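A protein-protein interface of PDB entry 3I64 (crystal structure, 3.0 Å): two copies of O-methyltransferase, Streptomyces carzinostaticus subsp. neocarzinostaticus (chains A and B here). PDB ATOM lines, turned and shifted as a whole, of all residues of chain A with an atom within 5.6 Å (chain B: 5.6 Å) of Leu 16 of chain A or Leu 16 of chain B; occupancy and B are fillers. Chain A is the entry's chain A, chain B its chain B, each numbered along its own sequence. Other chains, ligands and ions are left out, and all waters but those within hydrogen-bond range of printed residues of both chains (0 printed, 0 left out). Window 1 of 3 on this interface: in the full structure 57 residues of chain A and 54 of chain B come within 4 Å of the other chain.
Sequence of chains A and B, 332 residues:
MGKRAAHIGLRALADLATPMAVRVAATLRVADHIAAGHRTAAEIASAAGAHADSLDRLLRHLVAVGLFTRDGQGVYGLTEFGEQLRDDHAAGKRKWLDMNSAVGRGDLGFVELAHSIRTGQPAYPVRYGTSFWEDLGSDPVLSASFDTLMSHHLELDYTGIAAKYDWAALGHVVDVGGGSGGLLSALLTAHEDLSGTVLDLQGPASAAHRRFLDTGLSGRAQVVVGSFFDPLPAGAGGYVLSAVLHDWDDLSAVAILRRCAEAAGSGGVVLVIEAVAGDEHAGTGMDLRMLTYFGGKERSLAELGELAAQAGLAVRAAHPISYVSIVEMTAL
The guanidinium group (NE) of Arg 23 of chain A lies within hydrogen-bond range of the backbone carbonyl oxygen (O) of Ala 14 of chain B, at 2.9 Å. NE of Arg 23 of chain B is in hydrogen-bond range of O of Ala 14 of chain A (2.7 Å).
OD2 of Asp 15 of chain B is in hydrogen-bond range of N of Thr 18 of chain B (2.9 Å). OD2 of Asp 15 of chain A sits close to N of Thr 18 of chain A, at 3.1 Å. N of Ala 17 of chain A sits at hydrogen-bond distance from OD1 of Asp 15 of chain A, at 3.0 Å. NH2 of Arg 23 of chain A is in salt-bridge range of OD2 of Asp 107 of chain A. NH2 of Arg 23 of chain B is in salt-bridge range of OD2 of Asp 107 of chain B, at 3.4 Å. OD1 of Asp 15 of chain B lies within hydrogen-bond range of N of Ala 17 of chain B (3.0 Å).
Among the printed residues, pairs that only touch across the chains: Phe 110 of chain A with Met 20 of chain B (2.8 Å), Met 20 of chain A with Phe 110 of chain B (2.9 Å), Leu 16 of chain A with Met 20 of chain B (3.1 Å), Asp 15 of chain A with Pro 19 of chain B (3.2 Å), Pro 19 of chain A with Asp 15 of chain B (3.4 Å), Phe 110 of chain A with Ala 17 of chain B (3.5 Å), Ala 14 of chain A with Pro 19 of chain B (3.5 Å), Pro 19 of chain A with Ala 14 of chain B (3.5 Å), Ala 17 of chain A with Phe 110 of chain B (3.6 Å), Arg 23 of chain A with Leu 16 of chain B (3.6 Å), Asp 107 of chain A with Leu 16 of chain B (3.6 Å), Pro 19 of chain A with Leu 16 of chain B (3.7 Å), Leu 16 of chain A with Arg 23 of chain B (3.7 Å), Leu 16 of chain A with Asp 107 of chain B (3.8 Å), Leu 108 of chain A with Leu 16 of chain B (3.9 Å), Leu 16 of chain A with Leu 16 of chain B (3.9 Å) and Leu 16 of chain A with Leu 108 of chain B (3.99 Å).
Printed residues of chain B within 4 Å of Leu 16 of chain A: Leu 16, Met 20, Arg 23, Asp 107 and Leu 108. Printed residues of chain B within 4 Å of Arg 23 of chain A: Ala 14 and Leu 16. Of the printed residues of chain B, Asp 107 of chain A touches Leu 16 (3.6 Å). Of chain A, only Leu 16 (3.9 Å), Pro 19 (3.7 Å), Arg 23 (3.6 Å), Asp 107 (3.6 Å) and Leu 108 (3.9 Å) come within 4 Å of Leu 16 of chain B. Thr 18 of chain B touches none of the printed residues of chain A. Printed residues of chain A within 4 Å of Leu 108 of chain B: Leu 16. The nearest printed residue of chain B that does not touch Leu 16 of chain A is Pro 19 of chain B (4.02 Å). The nearest residue of chain A that does not touch Leu 16 of chain B is Met 20 of chain A (4.04 Å).
Printed residues of chain A that touch a printed residue of chain B: Ala 14, Asp 15, Leu 16, Ala 17, Pro 19, Met 20, Arg 23, Asp 107, Leu 108 and Phe 110. Hydrophobic or aromatic side chains of chain A that line the printed part of chain B: Leu 16, Ala 17, Pro 19, Met 20, Leu 108 and Phe 110. Of the 12 printed residues of chain B, 10 touch a printed residue of chain A. Hydrophobic or aromatic side chains of chain B within 4 Å of the printed part of chain A: Leu 16, Ala 17, Pro 19, Met 20, Leu 108 and Phe 110.
Asp 15 of chain A touches Pro 19 of chain B, and with the chains exchanged Pro 19 of chain A touches Asp 15 of chain B. Leu 16 of chain A touches its own counterpart, Leu 16 of chain B. Leu 16 of chain A touches Arg 23 of chain B, and with the chains exchanged Arg 23 of chain A touches Leu 16 of chain B. Met 20 of chain A touches Phe 110 of chain B, and with the chains exchanged Phe 110 of chain A touches Met 20 of chain B. Of the 19 pairs that touch across the chains among the printed residues, 17 have their exchanged pair printed and touching as well.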
ATOM      1  N   ALA A  14     -33.613  10.192   4.910  1.00  0.00           N
ATOM      2  CA  ALA A  14     -32.258   9.951   5.381  1.00  0.00           C
ATOM      3  C   ALA A  14     -31.262  10.966   4.854  1.00  0.00           C
ATOM      4  O   ALA A  14     -30.061  10.870   5.122  1.00  0.00           O
ATOM      5  CB  ALA A  14     -31.828   8.544   4.980  1.00  0.00           C
ATOM      6  N   ASP A  15     -31.769  11.943   4.110  1.00  0.00           N
ATOM      7  CA  ASP A  15     -30.936  12.984   3.515  1.00  0.00           C
ATOM      8  C   ASP A  15     -30.114  13.799   4.495  1.00  0.00           C
ATOM      9  O   ASP A  15     -30.613  14.251   5.526  1.00  0.00           O
ATOM     10  CB  ASP A  15     -31.795  13.940   2.692  1.00  0.00           C
ATOM     11  CG  ASP A  15     -31.025  15.170   2.242  1.00  0.00           C
ATOM     12  OD1 ASP A  15     -29.905  15.027   1.698  1.00  0.00           O
ATOM     13  OD2 ASP A  15     -31.546  16.288   2.428  1.00  0.00           O
ATOM     14  N   LEU A  16     -28.847  13.995   4.155  1.00  0.00           N
ATOM     15  CA  LEU A  16     -27.955  14.781   4.986  1.00  0.00           C
ATOM     16  C   LEU A  16     -27.604  16.101   4.301  1.00  0.00           C
ATOM     17  O   LEU A  16     -27.498  17.136   4.953  1.00  0.00           O
ATOM     18  CB  LEU A  16     -26.696  13.984   5.301  1.00  0.00           C
ATOM     19  CG  LEU A  16     -26.942  12.940   6.384  1.00  0.00           C
ATOM     20  CD1 LEU A  16     -25.683  12.181   6.657  1.00  0.00           C
ATOM     21  CD2 LEU A  16     -27.428  13.620   7.647  1.00  0.00           C
ATOM     22  N   ALA A  17     -27.449  16.067   2.984  1.00  0.00           N
ATOM     23  CA  ALA A  17     -27.118  17.265   2.229  1.00  0.00           C
ATOM     24  C   ALA A  17     -27.938  18.481   2.639  1.00  0.00           C
ATOM     25  O   ALA A  17     -27.385  19.540   2.897  1.00  0.00           O
ATOM     26  CB  ALA A  17     -27.292  17.015   0.749  1.00  0.00           C
ATOM     27  N   THR A  18     -29.253  18.340   2.712  1.00  0.00           N
ATOM     28  CA  THR A  18     -30.072  19.488   3.074  1.00  0.00           C
ATOM     29  C   THR A  18     -29.869  20.004   4.502  1.00  0.00           C
ATOM     30  O   THR A  18     -29.567  21.187   4.702  1.00  0.00           O
ATOM     31  CB  THR A  18     -31.566  19.203   2.800  1.00  0.00           C
ATOM     32  OG1 THR A  18     -31.822  19.403   1.404  1.00  0.00           O
ATOM     33  CG2 THR A  18     -32.464  20.119   3.613  1.00  0.00           C
ATOM     34  N   PRO A  19     -30.027  19.137   5.512  1.00  0.00           N
ATOM     35  CA  PRO A  19     -29.841  19.599   6.895  1.00  0.00           C
ATOM     36  C   PRO A  19     -28.511  20.337   7.071  1.00  0.00           C
ATOM     37  O   PRO A  19     -28.441  21.394   7.697  1.00  0.00           O
ATOM     38  CB  PRO A  19     -29.905  18.302   7.699  1.00  0.00           C
ATOM     39  CG  PRO A  19     -30.884  17.487   6.915  1.00  0.00           C
ATOM     40  CD  PRO A  19     -30.433  17.722   5.480  1.00  0.00           C
ATOM     41  N   MET A  20     -27.460  19.762   6.500  1.00  0.00           N
ATOM     42  CA  MET A  20     -26.129  20.335   6.563  1.00  0.00           C
ATOM     43  C   MET A  20     -26.087  21.667   5.814  1.00  0.00           C
ATOM     44  O   MET A  20     -25.497  22.630   6.290  1.00  0.00           O
ATOM     45  CB  MET A  20     -25.132  19.352   5.956  1.00  0.00           C
ATOM     46  CG  MET A  20     -24.000  18.946   6.879  1.00  0.00           C
ATOM     47  SD  MET A  20     -24.450  18.794   8.622  1.00  0.00           S
ATOM     48  CE  MET A  20     -23.259  19.913   9.265  1.00  0.00           C
ATOM     49  N   ALA A  21     -26.706  21.717   4.637  1.00  0.00           N
ATOM     50  CA  ALA A  21     -26.747  22.944   3.835  1.00  0.00           C
ATOM     51  C   ALA A  21     -27.427  24.073   4.608  1.00  0.00           C
ATOM     52  O   ALA A  21     -27.034  25.235   4.490  1.00  0.00           O
ATOM     53  CB  ALA A  21     -27.499  22.700   2.518  1.00  0.00           C
ATOM     54  N   ARG A  23     -27.625  24.287   7.992  1.00  0.00           N
ATOM     55  CA  ARG A  23     -26.722  24.630   9.082  1.00  0.00           C
ATOM     56  C   ARG A  23     -25.532  25.457   8.608  1.00  0.00           C
ATOM     57  O   ARG A  23     -25.021  26.291   9.341  1.00  0.00           O
ATOM     58  CB  ARG A  23     -26.263  23.352   9.789  1.00  0.00           C
ATOM     59  CG  ARG A  23     -27.413  22.665  10.535  1.00  0.00           C
ATOM     60  CD  ARG A  23     -27.061  21.293  11.069  1.00  0.00           C
ATOM     61  NE  ARG A  23     -28.212  20.673  11.716  1.00  0.00           N
ATOM     62  CZ  ARG A  23     -28.540  20.846  12.992  1.00  0.00           C
ATOM     63  NH1 ARG A  23     -27.798  21.622  13.770  1.00  0.00           N
ATOM     64  NH2 ARG A  23     -29.614  20.249  13.491  1.00  0.00           N
ATOM     65  N   ASP A 107     -24.650  18.993  17.882  1.00  0.00           N
ATOM     66  CA  ASP A 107     -25.585  18.201  17.091  1.00  0.00           C
ATOM     67  C   ASP A 107     -24.876  17.459  15.971  1.00  0.00           C
ATOM     68  O   ASP A 107     -25.348  16.421  15.526  1.00  0.00           O
ATOM     69  CB  ASP A 107     -26.694  19.088  16.520  1.00  0.00           C
ATOM     70  CG  ASP A 107     -27.884  19.226  17.472  1.00  0.00           C
ATOM     71  OD1 ASP A 107     -27.740  18.916  18.682  1.00  0.00           O
ATOM     72  OD2 ASP A 107     -28.966  19.652  17.002  1.00  0.00           O
ATOM     73  N   LEU A 108     -23.748  17.984  15.504  1.00  0.00           N
ATOM     74  CA  LEU A 108     -23.007  17.295  14.457  1.00  0.00           C
ATOM     75  C   LEU A 108     -22.516  15.971  15.035  1.00  0.00           C
ATOM     76  O   LEU A 108     -22.018  15.111  14.322  1.00  0.00           O
ATOM     77  CB  LEU A 108     -21.812  18.126  13.998  1.00  0.00           C
ATOM     78  CG  LEU A 108     -22.106  19.498  13.395  1.00  0.00           C
ATOM     79  CD1 LEU A 108     -20.840  20.094  12.778  1.00  0.00           C
ATOM     80  CD2 LEU A 108     -23.180  19.356  12.338  1.00  0.00           C
ATOM     81  N   PHE A 110     -24.304  13.800  16.041  1.00  0.00           N
ATOM     82  CA  PHE A 110     -25.289  12.817  15.632  1.00  0.00           C
ATOM     83  C   PHE A 110     -24.681  11.924  14.571  1.00  0.00           C
ATOM     84  O   PHE A 110     -25.093  10.779  14.407  1.00  0.00           O
ATOM     85  CB  PHE A 110     -26.535  13.502  15.065  1.00  0.00           C
ATOM     86  CG  PHE A 110     -27.617  13.695  16.068  1.00  0.00           C
ATOM     87  CD1 PHE A 110     -28.091  14.965  16.364  1.00  0.00           C
ATOM     88  CD2 PHE A 110     -28.160  12.602  16.736  1.00  0.00           C
ATOM     89  CE1 PHE A 110     -29.094  15.147  17.319  1.00  0.00           C
ATOM     90  CE2 PHE A 110     -29.165  12.769  17.690  1.00  0.00           C
ATOM     91  CZ  PHE A 110     -29.630  14.044  17.983  1.00  0.00           C
ATOM     92  N   ALA B  14     -33.674  21.226   9.244  1.00  0.00           N
ATOM     93  CA  ALA B  14     -32.250  21.152   9.545  1.00  0.00           C
ATOM     94  C   ALA B  14     -31.919  20.001  10.475  1.00  0.00           C
ATOM     95  O   ALA B  14     -30.754  19.754  10.786  1.00  0.00           O
ATOM     96  CB  ALA B  14     -31.787  22.468  10.163  1.00  0.00           C
ATOM     97  N   ASP B  15     -32.953  19.303  10.927  1.00  0.00           N
ATOM     98  CA  ASP B  15     -32.773  18.171  11.830  1.00  0.00           C
ATOM     99  C   ASP B  15     -31.786  17.138  11.307  1.00  0.00           C
ATOM    100  O   ASP B  15     -31.800  16.799  10.122  1.00  0.00           O
ATOM    101  CB  ASP B  15     -34.108  17.475  12.082  1.00  0.00           C
ATOM    102  CG  ASP B  15     -33.940  16.158  12.819  1.00  0.00           C
ATOM    103  OD1 ASP B  15     -33.323  16.159  13.911  1.00  0.00           O
ATOM    104  OD2 ASP B  15     -34.422  15.125  12.307  1.00  0.00           O
ATOM    105  N   LEU B  16     -30.937  16.633  12.195  1.00  0.00           N
ATOM    106  CA  LEU B  16     -29.968  15.609  11.820  1.00  0.00           C
ATOM    107  C   LEU B  16     -30.350  14.279  12.467  1.00  0.00           C
ATOM    108  O   LEU B  16     -30.150  13.216  11.889  1.00  0.00           O
ATOM    109  CB  LEU B  16     -28.564  16.000  12.273  1.00  0.00           C
ATOM    110  CG  LEU B  16     -27.845  17.107  11.519  1.00  0.00           C
ATOM    111  CD1 LEU B  16     -26.567  17.401  12.237  1.00  0.00           C
ATOM    112  CD2 LEU B  16     -27.577  16.701  10.096  1.00  0.00           C
ATOM    113  N   ALA B  17     -30.906  14.350  13.669  1.00  0.00           N
ATOM    114  CA  ALA B  17     -31.308  13.162  14.403  1.00  0.00           C
ATOM    115  C   ALA B  17     -32.071  12.153  13.562  1.00  0.00           C
ATOM    116  O   ALA B  17     -31.738  10.978  13.565  1.00  0.00           O
ATOM    117  CB  ALA B  17     -32.136  13.552  15.613  1.00  0.00           C
ATOM    118  N   THR B  18     -33.088  12.592  12.837  1.00  0.00           N
ATOM    119  CA  THR B  18     -33.859  11.651  12.039  1.00  0.00           C
ATOM    120  C   THR B  18     -33.082  11.001  10.899  1.00  0.00           C
ATOM    121  O   THR B  18     -33.023   9.775  10.811  1.00  0.00           O
ATOM    122  CB  THR B  18     -35.154  12.308  11.500  1.00  0.00           C
ATOM    123  OG1 THR B  18     -36.133  12.303  12.541  1.00  0.00           O
ATOM    124  CG2 THR B  18     -35.709  11.555  10.301  1.00  0.00           C
ATOM    125  N   PRO B  19     -32.478  11.802  10.009  1.00  0.00           N
ATOM    126  CA  PRO B  19     -31.735  11.162   8.916  1.00  0.00           C
ATOM    127  C   PRO B  19     -30.624  10.230   9.401  1.00  0.00           C
ATOM    128  O   PRO B  19     -30.299   9.242   8.758  1.00  0.00           O
ATOM    129  CB  PRO B  19     -31.219  12.351   8.092  1.00  0.00           C
ATOM    130  CG  PRO B  19     -31.207  13.485   9.062  1.00  0.00           C
ATOM    131  CD  PRO B  19     -32.452  13.269   9.882  1.00  0.00           C
ATOM    132  N   MET B  20     -30.063  10.547  10.555  1.00  0.00           N
ATOM    133  CA  MET B  20     -29.006   9.748  11.137  1.00  0.00           C
ATOM    134  C   MET B  20     -29.626   8.475  11.719  1.00  0.00           C
ATOM    135  O   MET B  20     -29.070   7.398  11.606  1.00  0.00           O
ATOM    136  CB  MET B  20     -28.312  10.573  12.220  1.00  0.00           C
ATOM    137  CG  MET B  20     -26.808  10.427  12.267  1.00  0.00           C
ATOM    138  SD  MET B  20     -26.040  10.254  10.646  1.00  0.00           S
ATOM    139  CE  MET B  20     -26.307  11.858   9.971  1.00  0.00           C
ATOM    140  N   ALA B  21     -30.788   8.613  12.342  1.00  0.00           N
ATOM    141  CA  ALA B  21     -31.508   7.482  12.924  1.00  0.00           C
ATOM    142  C   ALA B  21     -31.938   6.496  11.837  1.00  0.00           C
ATOM    143  O   ALA B  21     -31.951   5.282  12.058  1.00  0.00           O
ATOM    144  CB  ALA B  21     -32.746   7.976  13.685  1.00  0.00           C
ATOM    145  N   ARG B  23     -30.404   6.094   8.893  1.00  0.00           N
ATOM    146  CA  ARG B  23     -29.181   5.482   8.402  1.00  0.00           C
ATOM    147  C   ARG B  23     -28.650   4.434   9.356  1.00  0.00           C
ATOM    148  O   ARG B  23     -28.077   3.442   8.927  1.00  0.00           O
ATOM    149  CB  ARG B  23     -28.127   6.558   8.138  1.00  0.00           C
ATOM    150  CG  ARG B  23     -28.451   7.398   6.911  1.00  0.00           C
ATOM    151  CD  ARG B  23     -27.491   8.539   6.733  1.00  0.00           C
ATOM    152  NE  ARG B  23     -27.889   9.379   5.611  1.00  0.00           N
ATOM    153  CZ  ARG B  23     -27.456   9.227   4.364  1.00  0.00           C
ATOM    154  NH1 ARG B  23     -26.599   8.262   4.057  1.00  0.00           N
ATOM    155  NH2 ARG B  23     -27.885  10.045   3.416  1.00  0.00           N
ATOM    156  N   ASP B 107     -21.351   9.666   2.643  1.00  0.00           N
ATOM    157  CA  ASP B 107     -22.344  10.718   2.857  1.00  0.00           C
ATOM    158  C   ASP B 107     -22.209  11.373   4.227  1.00  0.00           C
ATOM    159  O   ASP B 107     -22.669  12.492   4.428  1.00  0.00           O
ATOM    160  CB  ASP B 107     -23.761  10.168   2.679  1.00  0.00           C
ATOM    161  CG  ASP B 107     -24.240  10.268   1.241  1.00  0.00           C
ATOM    162  OD1 ASP B 107     -23.368  10.406   0.346  1.00  0.00           O
ATOM    163  OD2 ASP B 107     -25.477  10.204   1.013  1.00  0.00           O
ATOM    164  N   LEU B 108     -21.598  10.675   5.177  1.00  0.00           N
ATOM    165  CA  LEU B 108     -21.405  11.256   6.491  1.00  0.00           C
ATOM    166  C   LEU B 108     -20.362  12.348   6.349  1.00  0.00           C
ATOM    167  O   LEU B 108     -20.112  13.107   7.274  1.00  0.00           O
ATOM    168  CB  LEU B 108     -20.892  10.215   7.474  1.00  0.00           C
ATOM    169  CG  LEU B 108     -21.766   8.999   7.728  1.00  0.00           C
ATOM    170  CD1 LEU B 108     -21.124   8.185   8.851  1.00  0.00           C
ATOM    171  CD2 LEU B 108     -23.185   9.428   8.115  1.00  0.00           C
ATOM    172  N   PHE B 110     -20.705  14.777   4.807  1.00  0.00           N
ATOM    173  CA  PHE B 110     -21.474  15.995   4.715  1.00  0.00           C
ATOM    174  C   PHE B 110     -21.318  16.830   5.985  1.00  0.00           C
ATOM    175  O   PHE B 110     -21.442  18.051   5.918  1.00  0.00           O
ATOM    176  CB  PHE B 110     -22.956  15.681   4.458  1.00  0.00           C
ATOM    177  CG  PHE B 110     -23.337  15.715   3.007  1.00  0.00           C
ATOM    178  CD1 PHE B 110     -23.804  14.576   2.365  1.00  0.00           C
ATOM    179  CD2 PHE B 110     -23.206  16.892   2.266  1.00  0.00           C
ATOM    180  CE1 PHE B 110     -24.131  14.602   0.998  1.00  0.00           C
ATOM    181  CE2 PHE B 110     -23.530  16.930   0.906  1.00  0.00           C
ATOM    182  CZ  PHE B 110     -23.991  15.782   0.274  1.00  0.00           C
